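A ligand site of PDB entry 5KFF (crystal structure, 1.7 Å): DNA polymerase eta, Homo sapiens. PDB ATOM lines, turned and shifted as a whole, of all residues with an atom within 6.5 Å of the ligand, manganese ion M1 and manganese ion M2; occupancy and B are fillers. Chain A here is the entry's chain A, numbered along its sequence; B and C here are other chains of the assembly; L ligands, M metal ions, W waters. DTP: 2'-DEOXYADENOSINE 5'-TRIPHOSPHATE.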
ATOM      1  N   ASP A  16     -31.320 -26.890   2.323  1.00  0.00           N
ATOM      2  CA  ASP A  16     -30.514 -27.105   3.509  1.00  0.00           C
ATOM      3  C   ASP A  16     -29.669 -28.355   3.433  1.00  0.00           C
ATOM      4  O   ASP A  16     -30.167 -29.366   3.268  1.00  0.00           O
ATOM      5  CB  ASP A  16     -31.379 -27.227   4.738  1.00  0.00           C
ATOM      6  CG  ASP A  16     -30.611 -27.396   5.965  1.00  0.00           C
ATOM      7  OD1 ASP A  16     -30.261 -28.492   6.219  1.00  0.00           O
ATOM      8  OD2 ASP A  16     -30.400 -26.396   6.554  1.00  0.00           O
ATOM      9  N   MET A  17     -28.380 -28.211   3.623  1.00  0.00           N
ATOM     10  CA  MET A  17     -27.490 -29.387   3.476  1.00  0.00           C
ATOM     11  C   MET A  17     -27.751 -30.459   4.554  1.00  0.00           C
ATOM     12  O   MET A  17     -28.012 -30.120   5.708  1.00  0.00           O
ATOM     13  CB  MET A  17     -26.017 -28.953   3.540  1.00  0.00           C
ATOM     14  CG  MET A  17     -25.665 -27.818   2.608  1.00  0.00           C
ATOM     15  SD  MET A  17     -26.115 -28.158   0.905  1.00  0.00           S
ATOM     16  CE  MET A  17     -25.060 -29.509   0.529  1.00  0.00           C
ATOM     17  N   ASP A  18     -27.695 -31.733   4.178  1.00  0.00           N
ATOM     18  CA  ASP A  18     -27.861 -32.811   5.173  1.00  0.00           C
ATOM     19  C   ASP A  18     -26.594 -33.045   5.984  1.00  0.00           C
ATOM     20  O   ASP A  18     -25.523 -33.212   5.398  1.00  0.00           O
ATOM     21  CB  ASP A  18     -28.200 -34.134   4.497  1.00  0.00           C
ATOM     22  CG  ASP A  18     -29.516 -34.087   3.730  1.00  0.00           C
ATOM     23  OD1 ASP A  18     -30.417 -33.303   4.112  1.00  0.00           O
ATOM     24  OD2 ASP A  18     -29.651 -34.856   2.770  1.00  0.00           O
ATOM     25  N   CYS A  19     -26.732 -33.055   7.317  1.00  0.00           N
ATOM     26  CA  CYS A  19     -25.616 -33.190   8.269  1.00  0.00           C
ATOM     27  C   CYS A  19     -24.320 -32.583   7.725  1.00  0.00           C
ATOM     28  O   CYS A  19     -23.335 -33.279   7.502  1.00  0.00           O
ATOM     29  CB  CYS A  19     -25.380 -34.642   8.710  1.00  0.00           C
ATOM     30  SG  CYS A  19     -25.201 -35.887   7.410  1.00  0.00           S
ATOM     31  N   PHE A  20     -24.359 -31.274   7.499  1.00  0.00           N
ATOM     32  CA  PHE A  20     -23.403 -30.612   6.624  1.00  0.00           C
ATOM     33  C   PHE A  20     -21.914 -30.837   6.967  1.00  0.00           C
ATOM     34  O   PHE A  20     -21.169 -31.316   6.113  1.00  0.00           O
ATOM     35  CB  PHE A  20     -23.698 -29.107   6.567  1.00  0.00           C
ATOM     36  CG  PHE A  20     -22.813 -28.351   5.615  1.00  0.00           C
ATOM     37  CD1 PHE A  20     -22.552 -28.860   4.351  1.00  0.00           C
ATOM     38  CD2 PHE A  20     -22.230 -27.154   5.992  1.00  0.00           C
ATOM     39  CE1 PHE A  20     -21.731 -28.143   3.456  1.00  0.00           C
ATOM     40  CE2 PHE A  20     -21.398 -26.445   5.109  1.00  0.00           C
ATOM     41  CZ  PHE A  20     -21.159 -26.949   3.840  1.00  0.00           C
ATOM     42  N   PHE A  21     -21.480 -30.509   8.194  1.00  0.00           N
ATOM     43  CA  PHE A  21     -20.051 -30.637   8.516  1.00  0.00           C
ATOM     44  C   PHE A  21     -19.613 -32.091   8.416  1.00  0.00           C
ATOM     45  O   PHE A  21     -18.488 -32.368   8.043  1.00  0.00           O
ATOM     46  CB  PHE A  21     -19.708 -30.102   9.926  1.00  0.00           C
ATOM     47  CG  PHE A  21     -19.803 -28.612  10.076  1.00  0.00           C
ATOM     48  CD1 PHE A  21     -20.438 -27.813   9.135  1.00  0.00           C
ATOM     49  CD2 PHE A  21     -19.236 -28.010  11.186  1.00  0.00           C
ATOM     50  CE1 PHE A  21     -20.520 -26.444   9.307  1.00  0.00           C
ATOM     51  CE2 PHE A  21     -19.314 -26.636  11.366  1.00  0.00           C
ATOM     52  CZ  PHE A  21     -19.958 -25.857  10.429  1.00  0.00           C
ATOM     53  N   VAL A  22     -20.515 -33.019   8.711  1.00  0.00           N
ATOM     54  CA  VAL A  22     -20.216 -34.436   8.553  1.00  0.00           C
ATOM     55  C   VAL A  22     -19.962 -34.777   7.066  1.00  0.00           C
ATOM     56  O   VAL A  22     -18.987 -35.455   6.746  1.00  0.00           O
ATOM     57  CB  VAL A  22     -21.347 -35.312   9.112  1.00  0.00           C
ATOM     58  CG1 VAL A  22     -21.266 -36.743   8.554  1.00  0.00           C
ATOM     59  CG2 VAL A  22     -21.310 -35.315  10.637  1.00  0.00           C
ATOM     60  N   GLN A  41     -15.650 -30.533  18.313  1.00  0.00           N
ATOM     61  CA  GLN A  41     -14.621 -29.497  18.479  1.00  0.00           C
ATOM     62  C   GLN A  41     -14.004 -29.640  19.856  1.00  0.00           C
ATOM     63  O   GLN A  41     -14.699 -29.897  20.841  1.00  0.00           O
ATOM     64  CB  GLN A  41     -15.178 -28.081  18.223  1.00  0.00           C
ATOM     65  CG  GLN A  41     -16.321 -27.631  19.076  1.00  0.00           C
ATOM     66  CD  GLN A  41     -17.009 -26.388  18.507  1.00  0.00           C
ATOM     67  OE1 GLN A  41     -16.648 -25.879  17.435  1.00  0.00           O
ATOM     68  NE2 GLN A  41     -17.997 -25.913  19.226  1.00  0.00           N
ATOM     69  N   ILE A  51     -20.911 -31.219  17.147  1.00  0.00           N
ATOM     70  CA  ILE A  51     -21.665 -30.147  16.489  1.00  0.00           C
ATOM     71  C   ILE A  51     -22.355 -30.610  15.208  1.00  0.00           C
ATOM     72  O   ILE A  51     -23.157 -29.860  14.643  1.00  0.00           O
ATOM     73  CB  ILE A  51     -20.780 -28.921  16.176  1.00  0.00           C
ATOM     74  CG1 ILE A  51     -19.597 -29.288  15.262  1.00  0.00           C
ATOM     75  CG2 ILE A  51     -20.304 -28.234  17.484  1.00  0.00           C
ATOM     76  CD1 ILE A  51     -18.857 -28.039  14.722  1.00  0.00           C
ATOM     77  N   ALA A  52     -22.074 -31.838  14.767  1.00  0.00           N
ATOM     78  CA  ALA A  52     -22.808 -32.423  13.626  1.00  0.00           C
ATOM     79  C   ALA A  52     -22.792 -33.946  13.679  1.00  0.00           C
ATOM     80  O   ALA A  52     -21.818 -34.553  14.130  1.00  0.00           O
ATOM     81  CB  ALA A  52     -22.228 -31.910  12.272  1.00  0.00           C
ATOM     82  N   VAL A  53     -23.887 -34.547  13.237  1.00  0.00           N
ATOM     83  CA  VAL A  53     -24.111 -35.989  13.423  1.00  0.00           C
ATOM     84  C   VAL A  53     -24.692 -36.630  12.163  1.00  0.00           C
ATOM     85  O   VAL A  53     -25.730 -36.172  11.635  1.00  0.00           O
ATOM     86  CB  VAL A  53     -25.086 -36.249  14.602  1.00  0.00           C
ATOM     87  CG1 VAL A  53     -25.215 -37.719  14.889  1.00  0.00           C
ATOM     88  CG2 VAL A  53     -24.662 -35.489  15.863  1.00  0.00           C
ATOM     89  N   TYR A  55     -26.708 -39.385   9.845  1.00  0.00           N
ATOM     90  CA  TYR A  55     -28.010 -39.997  10.071  1.00  0.00           C
ATOM     91  C   TYR A  55     -27.871 -41.414  10.629  1.00  0.00           C
ATOM     92  O   TYR A  55     -28.691 -41.819  11.449  1.00  0.00           O
ATOM     93  CB  TYR A  55     -28.846 -39.946   8.787  1.00  0.00           C
ATOM     94  CG  TYR A  55     -29.448 -38.567   8.631  1.00  0.00           C
ATOM     95  CD1 TYR A  55     -28.730 -37.534   8.048  1.00  0.00           C
ATOM     96  CD2 TYR A  55     -30.718 -38.288   9.127  1.00  0.00           C
ATOM     97  CE1 TYR A  55     -29.262 -36.247   7.955  1.00  0.00           C
ATOM     98  CE2 TYR A  55     -31.265 -37.009   9.034  1.00  0.00           C
ATOM     99  CZ  TYR A  55     -30.545 -35.992   8.448  1.00  0.00           C
ATOM    100  OH  TYR A  55     -31.087 -34.722   8.346  1.00  0.00           O
ATOM    101  N   ARG A  58     -27.391 -40.756  14.312  1.00  0.00           N
ATOM    102  CA  ARG A  58     -28.625 -40.298  14.959  1.00  0.00           C
ATOM    103  C   ARG A  58     -29.519 -41.469  15.384  1.00  0.00           C
ATOM    104  O   ARG A  58     -30.258 -41.377  16.371  1.00  0.00           O
ATOM    105  CB  ARG A  58     -29.403 -39.379  14.025  1.00  0.00           C
ATOM    106  CG  ARG A  58     -28.644 -38.140  13.676  1.00  0.00           C
ATOM    107  CD  ARG A  58     -29.446 -37.175  12.854  1.00  0.00           C
ATOM    108  NE  ARG A  58     -28.536 -36.169  12.283  1.00  0.00           N
ATOM    109  CZ  ARG A  58     -28.919 -35.079  11.634  1.00  0.00           C
ATOM    110  NH1 ARG A  58     -30.222 -34.830  11.493  1.00  0.00           N
ATOM    111  NH2 ARG A  58     -28.005 -34.239  11.156  1.00  0.00           N
ATOM    112  N   ARG A  64     -26.404 -33.304  18.477  1.00  0.00           N
ATOM    113  CA  ARG A  64     -25.635 -32.078  18.688  1.00  0.00           C
ATOM    114  C   ARG A  64     -25.647 -31.699  20.171  1.00  0.00           C
ATOM    115  O   ARG A  64     -26.619 -31.981  20.884  1.00  0.00           O
ATOM    116  CB  ARG A  64     -26.226 -30.958  17.813  1.00  0.00           C
ATOM    117  CG  ARG A  64     -25.673 -29.562  18.062  1.00  0.00           C
ATOM    118  CD  ARG A  64     -26.209 -28.593  17.025  1.00  0.00           C
ATOM    119  NE  ARG A  64     -25.750 -28.996  15.709  1.00  0.00           N
ATOM    120  CZ  ARG A  64     -26.521 -29.147  14.628  1.00  0.00           C
ATOM    121  NH1 ARG A  64     -27.833 -28.893  14.669  1.00  0.00           N
ATOM    122  NH2 ARG A  64     -25.961 -29.528  13.493  1.00  0.00           N
ATOM    123  N   LEU A  92     -13.271 -22.648  11.601  1.00  0.00           N
ATOM    124  CA  LEU A  92     -14.335 -23.239  10.760  1.00  0.00           C
ATOM    125  C   LEU A  92     -14.153 -22.985   9.271  1.00  0.00           C
ATOM    126  O   LEU A  92     -15.108 -23.121   8.493  1.00  0.00           O
ATOM    127  CB  LEU A  92     -15.697 -22.705  11.189  1.00  0.00           C
ATOM    128  CG  LEU A  92     -15.996 -22.828  12.677  1.00  0.00           C
ATOM    129  CD1 LEU A  92     -17.340 -22.194  13.005  1.00  0.00           C
ATOM    130  CD2 LEU A  92     -15.948 -24.284  13.085  1.00  0.00           C
ATOM    131  N   SER A 116     -27.810 -19.359   6.577  1.00  0.00           N
ATOM    132  CA  SER A 116     -26.852 -19.932   7.518  1.00  0.00           C
ATOM    133  C   SER A 116     -25.673 -20.482   6.752  1.00  0.00           C
ATOM    134  O   SER A 116     -25.642 -20.407   5.521  1.00  0.00           O
ATOM    135  CB  SER A 116     -27.478 -21.059   8.349  1.00  0.00           C
ATOM    136  OG  SER A 116     -27.516 -22.272   7.618  1.00  0.00           O
ATOM    137  N   ILE A 117     -24.725 -21.075   7.452  1.00  0.00           N
ATOM    138  CA  ILE A 117     -23.577 -21.677   6.774  1.00  0.00           C
ATOM    139  C   ILE A 117     -24.001 -22.811   5.823  1.00  0.00           C
ATOM    140  O   ILE A 117     -23.296 -23.129   4.872  1.00  0.00           O
ATOM    141  CB  ILE A 117     -22.533 -22.213   7.778  1.00  0.00           C
ATOM    142  CG1 ILE A 117     -21.168 -22.366   7.100  1.00  0.00           C
ATOM    143  CG2 ILE A 117     -23.001 -23.526   8.431  1.00  0.00           C
ATOM    144  CD1 ILE A 117     -20.041 -22.693   8.067  1.00  0.00           C
ATOM    145  N   ASP A 118     -25.163 -23.414   6.051  1.00  0.00           N
ATOM    146  CA  ASP A 118     -25.516 -24.567   5.218  1.00  0.00           C
ATOM    147  C   ASP A 118     -26.896 -24.462   4.562  1.00  0.00           C
ATOM    148  O   ASP A 118     -27.442 -25.474   4.085  1.00  0.00           O
ATOM    149  CB  ASP A 118     -25.444 -25.869   6.020  1.00  0.00           C
ATOM    150  CG  ASP A 118     -26.766 -26.233   6.703  1.00  0.00           C
ATOM    151  OD1 ASP A 118     -27.490 -25.361   7.263  1.00  0.00           O
ATOM    152  OD2 ASP A 118     -27.121 -27.435   6.591  1.00  0.00           O
ATOM    153  N   GLU A 119     -27.475 -23.258   4.495  1.00  0.00           N
ATOM    154  CA  GLU A 119     -28.776 -23.129   3.835  1.00  0.00           C
ATOM    155  C   GLU A 119     -29.011 -21.754   3.236  1.00  0.00           C
ATOM    156  O   GLU A 119     -28.448 -20.738   3.676  1.00  0.00           O
ATOM    157  CB  GLU A 119     -29.919 -23.468   4.800  1.00  0.00           C
ATOM    158  CG  GLU A 119     -30.233 -22.402   5.844  1.00  0.00           C
ATOM    159  CD  GLU A 119     -30.757 -23.009   7.139  1.00  0.00           C
ATOM    160  OE1 GLU A 119     -31.976 -23.044   7.337  1.00  0.00           O
ATOM    161  OE2 GLU A 119     -29.939 -23.516   7.941  1.00  0.00           O
ATOM    162  N   SER A 216     -31.561 -31.421   1.502  1.00  0.00           N
ATOM    163  CA  SER A 216     -33.005 -31.483   1.414  1.00  0.00           C
ATOM    164  C   SER A 216     -33.517 -30.114   1.037  1.00  0.00           C
ATOM    165  O   SER A 216     -32.745 -29.138   1.009  1.00  0.00           O
ATOM    166  CB  SER A 216     -33.595 -31.955   2.733  1.00  0.00           C
ATOM    167  OG  SER A 216     -33.052 -33.222   3.067  1.00  0.00           O
ATOM    168  N   LYS A 227     -39.056 -23.402   4.876  1.00  0.00           N
ATOM    169  CA  LYS A 227     -38.203 -23.998   5.860  1.00  0.00           C
ATOM    170  C   LYS A 227     -38.867 -25.154   6.625  1.00  0.00           C
ATOM    171  O   LYS A 227     -38.276 -26.147   6.873  1.00  0.00           O
ATOM    172  CB  LYS A 227     -37.754 -22.995   6.988  1.00  0.00           C
ATOM    173  CG  LYS A 227     -36.989 -23.329   8.143  1.00  0.00           C
ATOM    174  CD  LYS A 227     -35.631 -23.881   7.676  1.00  0.00           C
ATOM    175  CE  LYS A 227     -34.814 -24.406   8.878  1.00  0.00           C
ATOM    176  NZ  LYS A 227     -33.420 -24.876   8.574  1.00  0.00           N
ATOM    177  N   LYS A 234     -36.323 -35.121   5.488  1.00  0.00           N
ATOM    178  CA  LYS A 234     -34.875 -35.239   5.406  1.00  0.00           C
ATOM    179  C   LYS A 234     -34.395 -36.644   5.823  1.00  0.00           C
ATOM    180  O   LYS A 234     -35.062 -37.248   6.592  1.00  0.00           O
ATOM    181  CB  LYS A 234     -34.215 -34.131   6.243  1.00  0.00           C
ATOM    182  CG  LYS A 234     -34.549 -34.117   7.672  1.00  0.00           C
ATOM    183  CD  LYS A 234     -34.085 -32.818   8.353  1.00  0.00           C
ATOM    184  CE  LYS A 234     -34.546 -32.606   9.794  1.00  0.00           C
ATOM    185  NZ  LYS A 234     -33.378 -32.110  10.593  1.00  0.00           N
ATOM    186  N   PRO A 235     -33.277 -37.154   5.294  1.00  0.00           N
ATOM    187  CA  PRO A 235     -32.335 -36.491   4.399  1.00  0.00           C
ATOM    188  C   PRO A 235     -32.596 -36.765   2.934  1.00  0.00           C
ATOM    189  O   PRO A 235     -33.358 -37.677   2.604  1.00  0.00           O
ATOM    190  CB  PRO A 235     -31.003 -37.128   4.793  1.00  0.00           C
ATOM    191  CG  PRO A 235     -31.382 -38.549   5.121  1.00  0.00           C
ATOM    192  CD  PRO A 235     -32.766 -38.446   5.764  1.00  0.00           C
ATOM    193  P    DT B   8     -32.682 -23.164  13.435  1.00  0.00           P
ATOM    194  OP1  DT B   8     -33.510 -23.914  12.463  1.00  0.00           O
ATOM    195  OP2  DT B   8     -32.504 -23.684  14.826  1.00  0.00           O
ATOM    196  O5'  DT B   8     -31.188 -22.948  12.852  1.00  0.00           O
ATOM    197  C5'  DT B   8     -30.881 -22.475  11.469  1.00  0.00           C
ATOM    198  C4'  DT B   8     -29.377 -22.674  11.230  1.00  0.00           C
ATOM    199  O4'  DT B   8     -28.757 -22.047  12.375  1.00  0.00           O
ATOM    200  C3'  DT B   8     -29.049 -24.166  11.300  1.00  0.00           C
ATOM    201  O3'  DT B   8     -28.266 -24.573  10.160  1.00  0.00           O
ATOM    202  C2'  DT B   8     -28.267 -24.323  12.629  1.00  0.00           C
ATOM    203  C1'  DT B   8     -27.784 -22.920  12.908  1.00  0.00           C
ATOM    204  N1   DT B   8     -27.612 -22.615  14.359  1.00  0.00           N
ATOM    205  C2   DT B   8     -26.366 -22.267  14.813  1.00  0.00           C
ATOM    206  O2   DT B   8     -25.405 -22.184  14.080  1.00  0.00           O
ATOM    207  N3   DT B   8     -26.290 -22.003  16.159  1.00  0.00           N
ATOM    208  C4   DT B   8     -27.318 -22.060  17.076  1.00  0.00           C
ATOM    209  O4   DT B   8     -27.159 -21.804  18.281  1.00  0.00           O
ATOM    210  C5   DT B   8     -28.606 -22.439  16.534  1.00  0.00           C
ATOM    211  C7   DT B   8     -29.804 -22.518  17.436  1.00  0.00           C
ATOM    212  C6   DT B   8     -28.688 -22.678  15.215  1.00  0.00           C
ATOM    213  P    DT C   3     -22.332 -27.522  29.941  1.00  0.00           P
ATOM    214  OP1  DT C   3     -22.864 -26.395  30.744  1.00  0.00           O
ATOM    215  OP2  DT C   3     -22.678 -28.919  30.263  1.00  0.00           O
ATOM    216  O5'  DT C   3     -22.692 -27.250  28.402  1.00  0.00           O
ATOM    217  C5'  DT C   3     -22.018 -27.951  27.379  1.00  0.00           C
ATOM    218  C4'  DT C   3     -22.283 -27.305  26.041  1.00  0.00           C
ATOM    219  O4'  DT C   3     -23.579 -27.705  25.568  1.00  0.00           O
ATOM    220  C3'  DT C   3     -22.278 -25.772  26.074  1.00  0.00           C
ATOM    221  O3'  DT C   3     -21.268 -25.257  25.204  1.00  0.00           O
ATOM    222  C2'  DT C   3     -23.689 -25.374  25.632  1.00  0.00           C
ATOM    223  C1'  DT C   3     -24.178 -26.616  24.913  1.00  0.00           C
ATOM    224  N1   DT C   3     -25.647 -26.788  24.974  1.00  0.00           N
ATOM    225  C2   DT C   3     -26.368 -26.850  23.810  1.00  0.00           C
ATOM    226  O2   DT C   3     -25.855 -26.756  22.699  1.00  0.00           O
ATOM    227  N3   DT C   3     -27.714 -27.017  23.975  1.00  0.00           N
ATOM    228  C4   DT C   3     -28.404 -27.135  25.165  1.00  0.00           C
ATOM    229  O4   DT C   3     -29.619 -27.291  25.217  1.00  0.00           O
ATOM    230  C5   DT C   3     -27.586 -27.070  26.356  1.00  0.00           C
ATOM    231  C7   DT C   3     -28.220 -27.180  27.707  1.00  0.00           C
ATOM    232  C6   DT C   3     -26.260 -26.901  26.200  1.00  0.00           C
ATOM    233  P    DT C   4     -20.074 -24.387  25.835  1.00  0.00           P
ATOM    234  OP1  DT C   4     -19.347 -25.237  26.802  1.00  0.00           O
ATOM    235  OP2  DT C   4     -20.695 -23.112  26.262  1.00  0.00           O
ATOM    236  O5'  DT C   4     -19.116 -24.048  24.600  1.00  0.00           O
ATOM    237  C5'  DT C   4     -18.086 -24.940  24.171  1.00  0.00           C
ATOM    238  C4'  DT C   4     -17.638 -24.583  22.752  1.00  0.00           C
ATOM    239  O4'  DT C   4     -18.757 -24.805  21.867  1.00  0.00           O
ATOM    240  C3'  DT C   4     -17.259 -23.124  22.568  1.00  0.00           C
ATOM    241  O3'  DT C   4     -16.217 -23.047  21.617  1.00  0.00           O
ATOM    242  C2'  DT C   4     -18.551 -22.476  22.057  1.00  0.00           C
ATOM    243  C1'  DT C   4     -19.104 -23.611  21.197  1.00  0.00           C
ATOM    244  N1   DT C   4     -20.567 -23.639  20.980  1.00  0.00           N
ATOM    245  C2   DT C   4     -21.007 -24.053  19.761  1.00  0.00           C
ATOM    246  O2   DT C   4     -20.248 -24.314  18.836  1.00  0.00           O
ATOM    247  N3   DT C   4     -22.362 -24.121  19.620  1.00  0.00           N
ATOM    248  C4   DT C   4     -23.307 -23.857  20.571  1.00  0.00           C
ATOM    249  O4   DT C   4     -24.514 -23.956  20.337  1.00  0.00           O
ATOM    250  C5   DT C   4     -22.789 -23.451  21.861  1.00  0.00           C
ATOM    251  C7   DT C   4     -23.737 -23.118  22.976  1.00  0.00           C
ATOM    252  C6   DT C   4     -21.448 -23.369  22.013  1.00  0.00           C
ATOM    253  P    DA C   5     -15.588 -21.629  21.190  1.00  0.00           P
ATOM    254  OP1  DA C   5     -14.140 -21.869  20.994  1.00  0.00           O
ATOM    255  OP2  DA C   5     -16.074 -20.598  22.123  1.00  0.00           O
ATOM    256  O5'  DA C   5     -16.247 -21.348  19.770  1.00  0.00           O
ATOM    257  C5'  DA C   5     -15.975 -22.216  18.658  1.00  0.00           C
ATOM    258  C4'  DA C   5     -16.618 -21.660  17.400  1.00  0.00           C
ATOM    259  O4'  DA C   5     -18.067 -21.843  17.472  1.00  0.00           O
ATOM    260  C3'  DA C   5     -16.406 -20.161  17.182  1.00  0.00           C
ATOM    261  O3'  DA C   5     -16.258 -19.902  15.798  1.00  0.00           O
ATOM    262  C2'  DA C   5     -17.686 -19.547  17.724  1.00  0.00           C
ATOM    263  C1'  DA C   5     -18.695 -20.587  17.253  1.00  0.00           C
ATOM    264  N9   DA C   5     -19.952 -20.583  17.988  1.00  0.00           N
ATOM    265  C8   DA C   5     -20.127 -20.318  19.316  1.00  0.00           C
ATOM    266  N7   DA C   5     -21.375 -20.420  19.713  1.00  0.00           N
ATOM    267  C5   DA C   5     -22.067 -20.780  18.573  1.00  0.00           C
ATOM    268  C6   DA C   5     -23.434 -21.035  18.313  1.00  0.00           C
ATOM    269  N6   DA C   5     -24.385 -20.965  19.252  1.00  0.00           N
ATOM    270  N1   DA C   5     -23.774 -21.366  17.055  1.00  0.00           N
ATOM    271  C2   DA C   5     -22.826 -21.443  16.122  1.00  0.00           C
ATOM    272  N3   DA C   5     -21.514 -21.222  16.237  1.00  0.00           N
ATOM    273  C4   DA C   5     -21.198 -20.895  17.497  1.00  0.00           C
HETATM  274  PG  DTP L   1     -29.505 -31.630   9.158  1.00  0.00           P
HETATM  275  O1G DTP L   1     -29.712 -30.270   8.569  1.00  0.00           O
HETATM  276  O2G DTP L   1     -29.471 -32.737   8.114  1.00  0.00           O
HETATM  277  O3G DTP L   1     -30.493 -31.938  10.272  1.00  0.00           O
HETATM  278  PB  DTP L   1     -27.074 -30.375   9.927  1.00  0.00           P
HETATM  279  O1B DTP L   1     -26.815 -29.898   8.513  1.00  0.00           O
HETATM  280  O2B DTP L   1     -25.789 -30.826  10.611  1.00  0.00           O
HETATM  281  O3B DTP L   1     -28.073 -31.625   9.872  1.00  0.00           O
HETATM  282  PA  DTP L   1     -27.991 -27.760  10.599  1.00  0.00           P
HETATM  283  O1A DTP L   1     -28.561 -27.388   9.243  1.00  0.00           O
HETATM  284  O2A DTP L   1     -28.873 -27.269  11.721  1.00  0.00           O
HETATM  285  O3A DTP L   1     -27.822 -29.321  10.847  1.00  0.00           O
HETATM  286  O5' DTP L   1     -26.593 -27.055  10.769  1.00  0.00           O
HETATM  287  C5' DTP L   1     -25.666 -27.021   9.735  1.00  0.00           C
HETATM  288  C4' DTP L   1     -24.233 -27.055  10.255  1.00  0.00           C
HETATM  289  O4' DTP L   1     -24.031 -25.902  11.059  1.00  0.00           O
HETATM  290  C3' DTP L   1     -23.987 -28.218  11.085  1.00  0.00           C
HETATM  291  O3' DTP L   1     -23.509 -29.329  10.312  1.00  0.00           O
HETATM  292  C2' DTP L   1     -22.964 -27.781  12.047  1.00  0.00           C
HETATM  293  C1' DTP L   1     -23.280 -26.332  12.206  1.00  0.00           C
HETATM  294  N9  DTP L   1     -24.038 -26.070  13.376  1.00  0.00           N
HETATM  295  C8  DTP L   1     -25.381 -26.156  13.526  1.00  0.00           C
HETATM  296  N7  DTP L   1     -25.744 -25.824  14.762  1.00  0.00           N
HETATM  297  C5  DTP L   1     -24.642 -25.487  15.439  1.00  0.00           C
HETATM  298  C6  DTP L   1     -24.384 -25.064  16.743  1.00  0.00           C
HETATM  299  N6  DTP L   1     -25.464 -24.900  17.647  1.00  0.00           N
HETATM  300  N1  DTP L   1     -23.133 -24.812  17.115  1.00  0.00           N
HETATM  301  C2  DTP L   1     -22.085 -24.952  16.276  1.00  0.00           C
HETATM  302  N3  DTP L   1     -22.292 -25.372  14.996  1.00  0.00           N
HETATM  303  C4  DTP L   1     -23.547 -25.641  14.585  1.00  0.00           C
HETATM  304 MN    MN M   1     -29.316 -25.539   8.378  1.00  0.00          MN
HETATM  305 MN    MN M   2     -28.466 -28.896   7.458  1.00  0.00          MN
HETATM  306  O   HOH W   1     -28.156 -26.006  16.368  1.00  0.00           O
HETATM  307  O   HOH W   2     -30.381 -31.449  12.787  1.00  0.00           O
HETATM  308  O   HOH W   3     -25.920 -32.811  12.517  1.00  0.00           O
HETATM  309  O   HOH W   4     -25.835 -23.736  10.385  1.00  0.00           O
HETATM  310  O   HOH W   5     -31.787 -28.776   9.326  1.00  0.00           O
HETATM  311  O   HOH W   6     -31.040 -26.027   9.578  1.00  0.00           O
HETATM  312  O   HOH W   7     -23.400 -22.838  12.577  1.00  0.00           O
HETATM  313  O   HOH W   8     -19.917 -24.511  13.781  1.00  0.00           O
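OG of Ser 116 touches manganese ion M1, at 3.8 Å.
Within 4 Å of manganese ion M1: Asp 16, Ser 116, Asp 118, Glu 119 and DT 8 of chain B.
Manganese ion M2 is bound by O1G of the ligand (2.2 Å), OD2 of Asp 118 (2.2 Å), O of Met 17 (2.2 Å), O1B of the ligand (2.2 Å), OD1 of Asp 16 (2.2 Å) and O1A of the ligand (2.3 Å).
The backbone carbonyl oxygen of Ile 51 is in hydrogen-bond range of the guanidinium group of Arg 64, 2.9 Å away.
O of Val 53 is in hydrogen-bond range of NE of Arg 58, at 2.9 Å.
The side-chain carboxylate (OE1) of Glu 119 is in salt-bridge range of the side-chain amino group (NZ) of Lys 227, at 2.6 Å.
The backbone NH (N) of Asp 16 sits at hydrogen-bond distance from the backbone carbonyl oxygen (O) of Ser 216, at 3.0 Å.
NH1 of Arg 58 sits at hydrogen-bond distance from OH of Tyr 55 (3.3 Å).
N3 of DT 8 of chain B lies close to N1 of DA 5 of chain C (2.7 Å).
N of Glu 119 lies close to OG of Ser 116 (3.3 Å).
The side-chain carboxylate (OD1) of Asp 18 is in hydrogen-bond range of the side-chain hydroxyl (OG) of Ser 216 (2.8 Å).
Manganese ion M1 is bound by OD1 of Asp 118 (2.1 Å), water W6 (2.2 Å), OE2 of Glu 119 (2.2 Å), O1A of the ligand (2.2 Å), O3' of DT 8 of chain B (2.3 Å) and OD2 of Asp 16 (2.3 Å).
Within 4 Å of manganese ion M2: Asp 16, Met 17 and Asp 118.
CA of Asp 18 touches O2G of the ligand, 3.4 Å away.
Ile 51 touches the ligand (O to C2', 3.3 Å).
CB of Ala 52 touches O3' of the ligand, at 3.5 Å.
Ile 117 touches the ligand.
DA 5 of chain C touches the ligand.
Hydrophobic or aromatic side chains within 4 Å of the ligand: Phe 20, Phe 21, Ile 51, Ala 52, Tyr 55 and Ile 117.
17 residues have an atom within 4 Å of the ligand: Asp 16, Met 17, Asp 18, Cys 19, Phe 20, Phe 21, Ile 51, Ala 52, Tyr 55, Arg 58, Arg 64, Ile 117, Asp 118, Lys 234, DT 8 of chain B, DT 4 of chain C and DA 5 of chain C.
The nearest printed residue that does not touch the ligand is Glu 119 (4.3 Å).
Water W6 lies within hydrogen-bond range of NZ of Lys 227 and O2A of the ligand.
Water W1 bridges a nitrogen (N7) of the ligand (2.9 Å) and the guanidinium group (NH1) of Arg 64 (3.4 Å).
Water W7 bridges O2 of DT 8 of chain B (2.6 Å) and an oxygen (O4') of the ligand (3.5 Å).
O4 of DT 4 of chain C lies within hydrogen-bond range of a nitrogen (N6) of the ligand (3.0 Å).
O3G of the ligand is in salt-bridge range of NZ of Lys 234, 2.9 Å away.
The guanidinium group (NH1) of Arg 58 lies within salt-bridge range of an oxygen (O3G) of the ligand, at 3.2 Å.
N of Phe 20 is in hydrogen-bond range of O2B of the ligand (3.5 Å).
The side-chain hydroxyl (OH) of Tyr 55 sits at hydrogen-bond distance from an oxygen (O2G) of the ligand (2.6 Å).
N3 of DT 8 of chain B lies within hydrogen-bond range of N6 of the ligand (3.4 Å).
The backbone NH (N) of Phe 21 is in hydrogen-bond range of an oxygen (O3') of the ligand (3.2 Å).
NH2 of Arg 64 is in salt-bridge range of O2B of the ligand (3.2 Å).
The backbone NH (N) of Cys 19 sits at hydrogen-bond distance from an oxygen (O2G) of the ligand, 2.9 Å away.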
